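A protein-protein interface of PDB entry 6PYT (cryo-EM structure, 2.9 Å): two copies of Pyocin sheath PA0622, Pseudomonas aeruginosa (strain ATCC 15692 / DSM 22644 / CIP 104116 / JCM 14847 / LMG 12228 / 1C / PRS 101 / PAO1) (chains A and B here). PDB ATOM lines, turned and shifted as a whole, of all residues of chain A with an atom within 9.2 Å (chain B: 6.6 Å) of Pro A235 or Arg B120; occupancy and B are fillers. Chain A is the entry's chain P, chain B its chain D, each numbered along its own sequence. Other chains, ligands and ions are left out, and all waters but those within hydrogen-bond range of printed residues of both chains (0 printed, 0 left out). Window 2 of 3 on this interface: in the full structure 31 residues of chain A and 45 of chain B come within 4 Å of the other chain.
The backbone carbonyl oxygen (O) of Val A236 is in hydrogen-bond range of the side-chain hydroxyl (OG) of Ser B119, 3.3 Å away.
The backbone NH (N) of Lys B118 lies within hydrogen-bond range of the backbone carbonyl oxygen (O) of Ala B123, 3.4 Å away.
The backbone carbonyl oxygen of Glu A237 sits at hydrogen-bond distance from the backbone NH of Arg A246 (3.2 Å).
O of Pro A235 is in hydrogen-bond range of NH1 of Arg A246, at 3.1 Å.
Pro A235 touches Asp B116 (CB to CB, 3.6 Å).
Ser B119 touches Pro A235.
Pro A235 touches Arg B120 (CG to NE, 3.3 Å).
Arg A246 touches Arg B108.
Ser B119 touches Ile A259 (CB to O, 3.3 Å).
Arg A260 touches Lys B118 (CB to CE, 3.8 Å).
Asn B122 touches Arg A260.
CB of Asp A261 touches CG of Asn B122, 3.7 Å away.
Thr A232 touches none of the printed residues of chain B.
Pro A235 touches just these residues of chain B: Asp B116 (3.6 Å), Ser B119 (3.3 Å) and Arg B120 (3.3 Å).
Leu A250 touches none of the printed residues of chain B.
Of the printed residues of chain A, Lys B118 touches Arg A260.
Ser B119 touches three residues of chain A.
Of chain A, only Pro A235 comes within 4 Å of Arg B120.
Phe B121 touches none of the printed residues of chain A.
Of the printed residues of chain A, Asn B122 touches Arg A260 and Asp A261.
The nearest residue of chain A that does not touch Arg B120 is Ser A233 (4.8 Å).
Hydrophobic or aromatic side chains of chain A within 4 Å of the printed part of chain B: Pro A235.
Printed residues of chain B that touch a printed residue of chain A: Arg B108, Asp B116, Lys B118, Ser B119, Arg B120 and Asn B122.
No position is printed for both chains.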
ATOM      1  N   ASN A 160     -15.202  41.720 -17.119  1.00  0.00           N
ATOM      2  CA  ASN A 160     -15.556  40.509 -17.847  1.00  0.00           C
ATOM      3  C   ASN A 160     -14.466  40.105 -18.830  1.00  0.00           C
ATOM      4  O   ASN A 160     -14.534  39.018 -19.414  1.00  0.00           O
ATOM      5  CB  ASN A 160     -16.881  40.749 -18.590  1.00  0.00           C
ATOM      6  CG  ASN A 160     -17.598  39.461 -18.996  1.00  0.00           C
ATOM      7  OD1 ASN A 160     -17.160  38.354 -18.686  1.00  0.00           O
ATOM      8  ND2 ASN A 160     -18.717  39.611 -19.692  1.00  0.00           N
ATOM      9  N   SER A 161     -13.439  40.935 -18.995  1.00  0.00           N
ATOM     10  CA  SER A 161     -12.467  40.787 -20.066  1.00  0.00           C
ATOM     11  C   SER A 161     -11.450  39.698 -19.770  1.00  0.00           C
ATOM     12  O   SER A 161     -11.667  38.846 -18.906  1.00  0.00           O
ATOM     13  CB  SER A 161     -11.750  42.113 -20.318  1.00  0.00           C
ATOM     14  OG  SER A 161     -12.642  43.112 -20.774  1.00  0.00           O
ATOM     15  N   ASP A 163      -7.621  37.719 -19.063  1.00  0.00           N
ATOM     16  CA  ASP A 163      -6.777  37.591 -17.883  1.00  0.00           C
ATOM     17  C   ASP A 163      -5.881  38.800 -17.702  1.00  0.00           C
ATOM     18  O   ASP A 163      -5.596  39.191 -16.567  1.00  0.00           O
ATOM     19  CB  ASP A 163      -5.919  36.340 -17.996  1.00  0.00           C
ATOM     20  N   PRO A 183     -13.174  36.235 -12.228  1.00  0.00           N
ATOM     21  CA  PRO A 183     -14.129  35.693 -13.208  1.00  0.00           C
ATOM     22  C   PRO A 183     -15.554  35.767 -12.687  1.00  0.00           C
ATOM     23  O   PRO A 183     -15.836  35.395 -11.547  1.00  0.00           O
ATOM     24  CB  PRO A 183     -13.675  34.243 -13.387  1.00  0.00           C
ATOM     25  CG  PRO A 183     -12.315  34.207 -12.846  1.00  0.00           C
ATOM     26  CD  PRO A 183     -12.341  35.135 -11.708  1.00  0.00           C
ATOM     27  N   GLY A 184     -16.440  36.294 -13.518  1.00  0.00           N
ATOM     28  CA  GLY A 184     -17.821  36.411 -13.133  1.00  0.00           C
ATOM     29  C   GLY A 184     -18.515  35.068 -13.091  1.00  0.00           C
ATOM     30  O   GLY A 184     -18.069  34.079 -13.659  1.00  0.00           O
ATOM     31  N   GLN A 186     -21.705  32.733 -13.998  1.00  0.00           N
ATOM     32  CA  GLN A 186     -22.750  32.523 -14.986  1.00  0.00           C
ATOM     33  C   GLN A 186     -23.830  31.685 -14.307  1.00  0.00           C
ATOM     34  O   GLN A 186     -23.669  30.476 -14.138  1.00  0.00           O
ATOM     35  CB  GLN A 186     -22.157  31.832 -16.205  1.00  0.00           C
ATOM     36  CG  GLN A 186     -23.003  31.828 -17.433  1.00  0.00           C
ATOM     37  CD  GLN A 186     -22.283  31.173 -18.584  1.00  0.00           C
ATOM     38  OE1 GLN A 186     -21.201  30.615 -18.407  1.00  0.00           O
ATOM     39  NE2 GLN A 186     -22.858  31.259 -19.778  1.00  0.00           N
ATOM     40  N   THR A 230     -23.774  27.993 -11.981  1.00  0.00           N
ATOM     41  CA  THR A 230     -23.767  27.023 -13.063  1.00  0.00           C
ATOM     42  C   THR A 230     -22.543  27.115 -13.957  1.00  0.00           C
ATOM     43  O   THR A 230     -22.422  26.324 -14.895  1.00  0.00           O
ATOM     44  CB  THR A 230     -25.024  27.171 -13.932  1.00  0.00           C
ATOM     45  OG1 THR A 230     -25.100  28.507 -14.441  1.00  0.00           O
ATOM     46  CG2 THR A 230     -26.277  26.851 -13.142  1.00  0.00           C
ATOM     47  N   GLY A 231     -21.639  28.040 -13.696  1.00  0.00           N
ATOM     48  CA  GLY A 231     -20.465  28.205 -14.527  1.00  0.00           C
ATOM     49  C   GLY A 231     -19.879  29.578 -14.334  1.00  0.00           C
ATOM     50  O   GLY A 231     -20.447  30.433 -13.661  1.00  0.00           O
ATOM     51  N   THR A 232     -18.719  29.781 -14.939  1.00  0.00           N
ATOM     52  CA  THR A 232     -18.048  31.067 -14.880  1.00  0.00           C
ATOM     53  C   THR A 232     -18.124  31.757 -16.233  1.00  0.00           C
ATOM     54  O   THR A 232     -18.485  31.155 -17.245  1.00  0.00           O
ATOM     55  CB  THR A 232     -16.590  30.915 -14.443  1.00  0.00           C
ATOM     56  OG1 THR A 232     -15.871  30.174 -15.429  1.00  0.00           O
ATOM     57  CG2 THR A 232     -16.515  30.181 -13.129  1.00  0.00           C
ATOM     58  N   SER A 233     -17.788  33.050 -16.231  1.00  0.00           N
ATOM     59  CA  SER A 233     -17.833  33.827 -17.464  1.00  0.00           C
ATOM     60  C   SER A 233     -16.712  33.421 -18.402  1.00  0.00           C
ATOM     61  O   SER A 233     -16.883  33.430 -19.624  1.00  0.00           O
ATOM     62  CB  SER A 233     -17.750  35.319 -17.152  1.00  0.00           C
ATOM     63  OG  SER A 233     -18.883  35.742 -16.421  1.00  0.00           O
ATOM     64  N   ARG A 234     -15.561  33.069 -17.848  1.00  0.00           N
ATOM     65  CA  ARG A 234     -14.460  32.509 -18.592  1.00  0.00           C
ATOM     66  C   ARG A 234     -14.066  31.193 -17.941  1.00  0.00           C
ATOM     67  O   ARG A 234     -14.112  31.073 -16.713  1.00  0.00           O
ATOM     68  CB  ARG A 234     -13.267  33.457 -18.592  1.00  0.00           C
ATOM     69  CG  ARG A 234     -13.523  34.765 -19.280  1.00  0.00           C
ATOM     70  CD  ARG A 234     -12.287  35.618 -19.230  1.00  0.00           C
ATOM     71  NE  ARG A 234     -11.953  36.035 -17.872  1.00  0.00           N
ATOM     72  CZ  ARG A 234     -10.879  35.612 -17.214  1.00  0.00           C
ATOM     73  NH1 ARG A 234     -10.058  34.753 -17.792  1.00  0.00           N
ATOM     74  NH2 ARG A 234     -10.630  36.035 -15.985  1.00  0.00           N
ATOM     75  N   PRO A 235     -13.695  30.183 -18.723  1.00  0.00           N
ATOM     76  CA  PRO A 235     -13.245  28.919 -18.123  1.00  0.00           C
ATOM     77  C   PRO A 235     -11.861  29.111 -17.525  1.00  0.00           C
ATOM     78  O   PRO A 235     -10.932  29.533 -18.214  1.00  0.00           O
ATOM     79  CB  PRO A 235     -13.222  27.950 -19.311  1.00  0.00           C
ATOM     80  CG  PRO A 235     -13.988  28.628 -20.396  1.00  0.00           C
ATOM     81  CD  PRO A 235     -13.785  30.089 -20.190  1.00  0.00           C
ATOM     82  N   VAL A 236     -11.738  28.844 -16.241  1.00  0.00           N
ATOM     83  CA  VAL A 236     -10.478  29.028 -15.539  1.00  0.00           C
ATOM     84  C   VAL A 236      -9.814  27.671 -15.364  1.00  0.00           C
ATOM     85  O   VAL A 236     -10.463  26.674 -15.036  1.00  0.00           O
ATOM     86  CB  VAL A 236     -10.693  29.759 -14.202  1.00  0.00           C
ATOM     87  CG1 VAL A 236      -9.418  29.867 -13.404  1.00  0.00           C
ATOM     88  CG2 VAL A 236     -11.194  31.136 -14.476  1.00  0.00           C
ATOM     89  N   GLU A 237      -8.511  27.643 -15.589  1.00  0.00           N
ATOM     90  CA  GLU A 237      -7.746  26.455 -15.922  1.00  0.00           C
ATOM     91  C   GLU A 237      -6.741  26.195 -14.809  1.00  0.00           C
ATOM     92  O   GLU A 237      -5.682  26.828 -14.766  1.00  0.00           O
ATOM     93  CB  GLU A 237      -7.054  26.702 -17.256  1.00  0.00           C
ATOM     94  N   PHE A 238      -7.042  25.278 -13.904  1.00  0.00           N
ATOM     95  CA  PHE A 238      -6.040  24.860 -12.936  1.00  0.00           C
ATOM     96  C   PHE A 238      -5.381  23.571 -13.394  1.00  0.00           C
ATOM     97  O   PHE A 238      -5.973  22.493 -13.306  1.00  0.00           O
ATOM     98  CB  PHE A 238      -6.580  24.686 -11.528  1.00  0.00           C
ATOM     99  CG  PHE A 238      -5.545  24.138 -10.609  1.00  0.00           C
ATOM    100  CD1 PHE A 238      -4.405  24.873 -10.338  1.00  0.00           C
ATOM    101  CD2 PHE A 238      -5.677  22.878 -10.051  1.00  0.00           C
ATOM    102  CE1 PHE A 238      -3.424  24.371  -9.519  1.00  0.00           C
ATOM    103  CE2 PHE A 238      -4.695  22.372  -9.223  1.00  0.00           C
ATOM    104  CZ  PHE A 238      -3.567  23.123  -8.959  1.00  0.00           C
ATOM    105  N   CYS A 245      -0.978  28.432 -16.590  1.00  0.00           N
ATOM    106  CA  CYS A 245      -2.335  28.075 -16.218  1.00  0.00           C
ATOM    107  C   CYS A 245      -3.106  29.340 -15.889  1.00  0.00           C
ATOM    108  O   CYS A 245      -2.555  30.283 -15.322  1.00  0.00           O
ATOM    109  CB  CYS A 245      -2.315  27.150 -15.007  1.00  0.00           C
ATOM    110  SG  CYS A 245      -1.264  25.719 -15.237  1.00  0.00           S
ATOM    111  N   ARG A 246      -4.380  29.369 -16.267  1.00  0.00           N
ATOM    112  CA  ARG A 246      -5.180  30.561 -16.019  1.00  0.00           C
ATOM    113  C   ARG A 246      -5.468  30.743 -14.533  1.00  0.00           C
ATOM    114  O   ARG A 246      -5.529  31.877 -14.048  1.00  0.00           O
ATOM    115  CB  ARG A 246      -6.459  30.484 -16.845  1.00  0.00           C
ATOM    116  CG  ARG A 246      -7.363  31.675 -16.734  1.00  0.00           C
ATOM    117  CD  ARG A 246      -8.407  31.658 -17.827  1.00  0.00           C
ATOM    118  NE  ARG A 246      -7.801  31.944 -19.122  1.00  0.00           N
ATOM    119  CZ  ARG A 246      -8.446  31.880 -20.280  1.00  0.00           C
ATOM    120  NH1 ARG A 246      -9.725  31.540 -20.316  1.00  0.00           N
ATOM    121  NH2 ARG A 246      -7.812  32.165 -21.405  1.00  0.00           N
ATOM    122  N   ALA A 247      -5.595  29.646 -13.788  1.00  0.00           N
ATOM    123  CA  ALA A 247      -5.735  29.751 -12.343  1.00  0.00           C
ATOM    124  C   ALA A 247      -4.427  30.139 -11.671  1.00  0.00           C
ATOM    125  O   ALA A 247      -4.445  30.747 -10.598  1.00  0.00           O
ATOM    126  CB  ALA A 247      -6.235  28.436 -11.768  1.00  0.00           C
ATOM    127  N   LEU A 250      -3.598  34.038 -12.482  1.00  0.00           N
ATOM    128  CA  LEU A 250      -4.358  35.001 -11.707  1.00  0.00           C
ATOM    129  C   LEU A 250      -4.024  34.938 -10.226  1.00  0.00           C
ATOM    130  O   LEU A 250      -4.138  35.953  -9.538  1.00  0.00           O
ATOM    131  CB  LEU A 250      -5.850  34.793 -11.943  1.00  0.00           C
ATOM    132  CG  LEU A 250      -6.262  35.139 -13.374  1.00  0.00           C
ATOM    133  CD1 LEU A 250      -7.702  34.802 -13.663  1.00  0.00           C
ATOM    134  CD2 LEU A 250      -6.010  36.603 -13.648  1.00  0.00           C
ATOM    135  N   THR A 257      -9.825  32.867  -7.970  1.00  0.00           N
ATOM    136  CA  THR A 257     -10.592  32.436  -9.128  1.00  0.00           C
ATOM    137  C   THR A 257     -11.630  31.407  -8.712  1.00  0.00           C
ATOM    138  O   THR A 257     -11.795  31.093  -7.534  1.00  0.00           O
ATOM    139  CB  THR A 257      -9.694  31.837 -10.214  1.00  0.00           C
ATOM    140  OG1 THR A 257      -8.977  30.715  -9.687  1.00  0.00           O
ATOM    141  CG2 THR A 257      -8.723  32.849 -10.713  1.00  0.00           C
ATOM    142  N   ILE A 258     -12.342  30.893  -9.710  1.00  0.00           N
ATOM    143  CA  ILE A 258     -13.300  29.804  -9.568  1.00  0.00           C
ATOM    144  C   ILE A 258     -12.944  28.776 -10.633  1.00  0.00           C
ATOM    145  O   ILE A 258     -12.944  29.103 -11.824  1.00  0.00           O
ATOM    146  CB  ILE A 258     -14.743  30.294  -9.739  1.00  0.00           C
ATOM    147  CG1 ILE A 258     -15.073  31.380  -8.717  1.00  0.00           C
ATOM    148  CG2 ILE A 258     -15.687  29.163  -9.548  1.00  0.00           C
ATOM    149  CD1 ILE A 258     -16.317  32.151  -9.032  1.00  0.00           C
ATOM    150  N   ILE A 259     -12.634  27.542 -10.226  1.00  0.00           N
ATOM    151  CA  ILE A 259     -11.725  26.700 -10.990  1.00  0.00           C
ATOM    152  C   ILE A 259     -12.385  25.466 -11.603  1.00  0.00           C
ATOM    153  O   ILE A 259     -12.044  25.106 -12.731  1.00  0.00           O
ATOM    154  CB  ILE A 259     -10.481  26.321 -10.161  1.00  0.00           C
ATOM    155  CG1 ILE A 259     -10.835  25.973  -8.713  1.00  0.00           C
ATOM    156  CG2 ILE A 259      -9.484  27.435 -10.251  1.00  0.00           C
ATOM    157  CD1 ILE A 259     -11.067  24.521  -8.437  1.00  0.00           C
ATOM    158  N   ARG A 260     -13.289  24.773 -10.915  1.00  0.00           N
ATOM    159  CA  ARG A 260     -13.699  23.472 -11.445  1.00  0.00           C
ATOM    160  C   ARG A 260     -15.208  23.399 -11.605  1.00  0.00           C
ATOM    161  O   ARG A 260     -15.926  24.307 -11.200  1.00  0.00           O
ATOM    162  CB  ARG A 260     -13.212  22.315 -10.559  1.00  0.00           C
ATOM    163  CG  ARG A 260     -13.910  22.192  -9.228  1.00  0.00           C
ATOM    164  CD  ARG A 260     -13.291  21.087  -8.392  1.00  0.00           C
ATOM    165  NE  ARG A 260     -13.464  19.778  -9.007  1.00  0.00           N
ATOM    166  CZ  ARG A 260     -14.521  18.992  -8.831  1.00  0.00           C
ATOM    167  NH1 ARG A 260     -15.512  19.369  -8.041  1.00  0.00           N
ATOM    168  NH2 ARG A 260     -14.582  17.820  -9.442  1.00  0.00           N
ATOM    169  N   ASP A 261     -15.647  22.349 -12.316  1.00  0.00           N
ATOM    170  CA  ASP A 261     -16.950  21.673 -12.175  1.00  0.00           C
ATOM    171  C   ASP A 261     -18.136  22.636 -12.250  1.00  0.00           C
ATOM    172  O   ASP A 261     -18.868  22.828 -11.276  1.00  0.00           O
ATOM    173  CB  ASP A 261     -16.970  20.863 -10.871  1.00  0.00           C
ATOM    174  N   ASP A 262     -18.307  23.234 -13.434  1.00  0.00           N
ATOM    175  CA  ASP A 262     -19.327  24.258 -13.706  1.00  0.00           C
ATOM    176  C   ASP A 262     -19.243  25.419 -12.718  1.00  0.00           C
ATOM    177  O   ASP A 262     -20.249  25.869 -12.168  1.00  0.00           O
ATOM    178  CB  ASP A 262     -20.740  23.662 -13.715  1.00  0.00           C
ATOM    179  N   GLY A 263     -18.024  25.893 -12.479  1.00  0.00           N
ATOM    180  CA  GLY A 263     -17.824  26.935 -11.497  1.00  0.00           C
ATOM    181  C   GLY A 263     -18.109  26.458 -10.088  1.00  0.00           C
ATOM    182  O   GLY A 263     -19.187  26.721  -9.568  1.00  0.00           O
ATOM    183  N   TYR A 264     -17.208  25.706  -9.471  1.00  0.00           N
ATOM    184  CA  TYR A 264     -17.580  25.014  -8.247  1.00  0.00           C
ATOM    185  C   TYR A 264     -16.910  25.584  -7.003  1.00  0.00           C
ATOM    186  O   TYR A 264     -17.562  25.706  -5.967  1.00  0.00           O
ATOM    187  CB  TYR A 264     -17.265  23.524  -8.406  1.00  0.00           C
ATOM    188  CG  TYR A 264     -17.905  22.584  -7.431  1.00  0.00           C
ATOM    189  CD1 TYR A 264     -19.280  22.407  -7.417  1.00  0.00           C
ATOM    190  CD2 TYR A 264     -17.134  21.800  -6.586  1.00  0.00           C
ATOM    191  CE1 TYR A 264     -19.878  21.521  -6.534  1.00  0.00           C
ATOM    192  CE2 TYR A 264     -17.717  20.905  -5.708  1.00  0.00           C
ATOM    193  CZ  TYR A 264     -19.090  20.772  -5.684  1.00  0.00           C
ATOM    194  OH  TYR A 264     -19.688  19.891  -4.814  1.00  0.00           O
ATOM    195  N   ASN B  44     -15.696  27.699 -32.409  1.00  0.00           N
ATOM    196  CA  ASN B  44     -14.633  27.514 -31.423  1.00  0.00           C
ATOM    197  C   ASN B  44     -15.172  27.476 -29.997  1.00  0.00           C
ATOM    198  O   ASN B  44     -14.657  28.135 -29.098  1.00  0.00           O
ATOM    199  CB  ASN B  44     -13.586  28.604 -31.591  1.00  0.00           C
ATOM    200  CG  ASN B  44     -12.832  28.471 -32.886  1.00  0.00           C
ATOM    201  OD1 ASN B  44     -12.447  27.374 -33.279  1.00  0.00           O
ATOM    202  ND2 ASN B  44     -12.630  29.588 -33.571  1.00  0.00           N
ATOM    203  N   VAL B  45     -16.205  26.667 -29.771  1.00  0.00           N
ATOM    204  CA  VAL B  45     -16.793  26.486 -28.458  1.00  0.00           C
ATOM    205  C   VAL B  45     -16.867  24.984 -28.180  1.00  0.00           C
ATOM    206  O   VAL B  45     -17.499  24.257 -28.952  1.00  0.00           O
ATOM    207  CB  VAL B  45     -18.188  27.115 -28.330  1.00  0.00           C
ATOM    208  CG1 VAL B  45     -18.825  26.716 -27.017  1.00  0.00           C
ATOM    209  CG2 VAL B  45     -18.102  28.624 -28.422  1.00  0.00           C
ATOM    210  N   PRO B  46     -16.240  24.486 -27.128  1.00  0.00           N
ATOM    211  CA  PRO B  46     -16.341  23.058 -26.822  1.00  0.00           C
ATOM    212  C   PRO B  46     -17.713  22.698 -26.288  1.00  0.00           C
ATOM    213  O   PRO B  46     -18.359  23.479 -25.591  1.00  0.00           O
ATOM    214  CB  PRO B  46     -15.256  22.848 -25.762  1.00  0.00           C
ATOM    215  CG  PRO B  46     -15.072  24.174 -25.146  1.00  0.00           C
ATOM    216  CD  PRO B  46     -15.309  25.178 -26.224  1.00  0.00           C
ATOM    217  N   ARG B 108     -10.390  31.190 -26.377  1.00  0.00           N
ATOM    218  CA  ARG B 108      -9.446  30.159 -26.784  1.00  0.00           C
ATOM    219  C   ARG B 108     -10.057  29.367 -27.926  1.00  0.00           C
ATOM    220  O   ARG B 108     -11.212  28.939 -27.837  1.00  0.00           O
ATOM    221  CB  ARG B 108      -9.112  29.232 -25.618  1.00  0.00           C
ATOM    222  CG  ARG B 108      -8.602  29.947 -24.393  1.00  0.00           C
ATOM    223  CD  ARG B 108      -8.189  28.954 -23.325  1.00  0.00           C
ATOM    224  NE  ARG B 108      -6.981  28.253 -23.736  1.00  0.00           N
ATOM    225  CZ  ARG B 108      -5.752  28.678 -23.464  1.00  0.00           C
ATOM    226  NH1 ARG B 108      -5.578  29.786 -22.762  1.00  0.00           N
ATOM    227  NH2 ARG B 108      -4.699  27.995 -23.885  1.00  0.00           N
ATOM    228  N   LEU B 115      -8.439  22.941 -23.284  1.00  0.00           N
ATOM    229  CA  LEU B 115      -8.040  23.307 -21.932  1.00  0.00           C
ATOM    230  C   LEU B 115      -9.194  23.897 -21.140  1.00  0.00           C
ATOM    231  O   LEU B 115      -9.118  23.967 -19.912  1.00  0.00           O
ATOM    232  CB  LEU B 115      -6.890  24.302 -21.989  1.00  0.00           C
ATOM    233  CG  LEU B 115      -5.635  23.724 -22.613  1.00  0.00           C
ATOM    234  CD1 LEU B 115      -4.607  24.811 -22.807  1.00  0.00           C
ATOM    235  CD2 LEU B 115      -5.106  22.620 -21.730  1.00  0.00           C
ATOM    236  N   ASP B 116     -10.250  24.322 -21.820  1.00  0.00           N
ATOM    237  CA  ASP B 116     -11.478  24.783 -21.204  1.00  0.00           C
ATOM    238  C   ASP B 116     -12.468  23.657 -20.975  1.00  0.00           C
ATOM    239  O   ASP B 116     -13.624  23.934 -20.666  1.00  0.00           O
ATOM    240  CB  ASP B 116     -12.126  25.852 -22.081  1.00  0.00           C
ATOM    241  N   GLY B 117     -12.047  22.402 -21.140  1.00  0.00           N
ATOM    242  CA  GLY B 117     -12.982  21.293 -21.030  1.00  0.00           C
ATOM    243  C   GLY B 117     -13.466  21.087 -19.609  1.00  0.00           C
ATOM    244  O   GLY B 117     -14.660  20.898 -19.367  1.00  0.00           O
ATOM    245  N   LYS B 118     -12.547  21.115 -18.655  1.00  0.00           N
ATOM    246  CA  LYS B 118     -12.925  21.297 -17.269  1.00  0.00           C
ATOM    247  C   LYS B 118     -13.256  22.771 -17.069  1.00  0.00           C
ATOM    248  O   LYS B 118     -12.790  23.625 -17.829  1.00  0.00           O
ATOM    249  CB  LYS B 118     -11.791  20.837 -16.354  1.00  0.00           C
ATOM    250  CG  LYS B 118     -12.160  20.643 -14.903  1.00  0.00           C
ATOM    251  CD  LYS B 118     -11.006  20.024 -14.144  1.00  0.00           C
ATOM    252  CE  LYS B 118     -11.360  19.768 -12.697  1.00  0.00           C
ATOM    253  NZ  LYS B 118     -10.213  19.171 -11.965  1.00  0.00           N
ATOM    254  N   SER B 119     -14.132  23.044 -16.091  1.00  0.00           N
ATOM    255  CA  SER B 119     -14.747  24.325 -15.709  1.00  0.00           C
ATOM    256  C   SER B 119     -15.817  24.788 -16.689  1.00  0.00           C
ATOM    257  O   SER B 119     -16.527  25.759 -16.417  1.00  0.00           O
ATOM    258  CB  SER B 119     -13.730  25.459 -15.522  1.00  0.00           C
ATOM    259  OG  SER B 119     -13.153  25.841 -16.751  1.00  0.00           O
ATOM    260  N   ARG B 120     -15.952  24.110 -17.817  1.00  0.00           N
ATOM    261  CA  ARG B 120     -17.142  24.221 -18.641  1.00  0.00           C
ATOM    262  C   ARG B 120     -18.052  23.024 -18.521  1.00  0.00           C
ATOM    263  O   ARG B 120     -19.260  23.168 -18.691  1.00  0.00           O
ATOM    264  CB  ARG B 120     -16.777  24.392 -20.118  1.00  0.00           C
ATOM    265  CG  ARG B 120     -16.329  25.757 -20.532  1.00  0.00           C
ATOM    266  CD  ARG B 120     -17.538  26.642 -20.652  1.00  0.00           C
ATOM    267  NE  ARG B 120     -17.178  27.996 -21.068  1.00  0.00           N
ATOM    268  CZ  ARG B 120     -17.051  28.371 -22.333  1.00  0.00           C
ATOM    269  NH1 ARG B 120     -17.236  27.489 -23.305  1.00  0.00           N
ATOM    270  NH2 ARG B 120     -16.726  29.621 -22.622  1.00  0.00           N
ATOM    271  N   PHE B 121     -17.494  21.838 -18.293  1.00  0.00           N
ATOM    272  CA  PHE B 121     -18.286  20.623 -18.286  1.00  0.00           C
ATOM    273  C   PHE B 121     -17.864  19.604 -17.241  1.00  0.00           C
ATOM    274  O   PHE B 121     -18.469  18.528 -17.199  1.00  0.00           O
ATOM    275  CB  PHE B 121     -18.233  19.954 -19.662  1.00  0.00           C
ATOM    276  CG  PHE B 121     -18.752  20.800 -20.773  1.00  0.00           C
ATOM    277  CD1 PHE B 121     -20.106  21.034 -20.908  1.00  0.00           C
ATOM    278  CD2 PHE B 121     -17.882  21.342 -21.696  1.00  0.00           C
ATOM    279  CE1 PHE B 121     -20.582  21.815 -21.935  1.00  0.00           C
ATOM    280  CE2 PHE B 121     -18.347  22.113 -22.720  1.00  0.00           C
ATOM    281  CZ  PHE B 121     -19.701  22.354 -22.841  1.00  0.00           C
ATOM    282  N   ASN B 122     -16.868  19.911 -16.401  1.00  0.00           N
ATOM    283  CA  ASN B 122     -16.245  18.982 -15.445  1.00  0.00           C
ATOM    284  C   ASN B 122     -15.725  17.733 -16.159  1.00  0.00           C
ATOM    285  O   ASN B 122     -15.980  16.596 -15.759  1.00  0.00           O
ATOM    286  CB  ASN B 122     -17.197  18.608 -14.303  1.00  0.00           C
ATOM    287  CG  ASN B 122     -16.481  18.005 -13.114  1.00  0.00           C
ATOM    288  OD1 ASN B 122     -15.258  18.016 -13.045  1.00  0.00           O
ATOM    289  ND2 ASN B 122     -17.242  17.409 -12.209  1.00  0.00           N
ATOM    290  N   ALA B 123     -15.000  17.955 -17.251  1.00  0.00           N
ATOM    291  CA  ALA B 123     -14.454  16.867 -18.060  1.00  0.00           C
ATOM    292  C   ALA B 123     -13.095  17.316 -18.584  1.00  0.00           C
ATOM    293  O   ALA B 123     -13.009  17.940 -19.641  1.00  0.00           O
ATOM    294  CB  ALA B 123     -15.403  16.503 -19.189  1.00  0.00           C
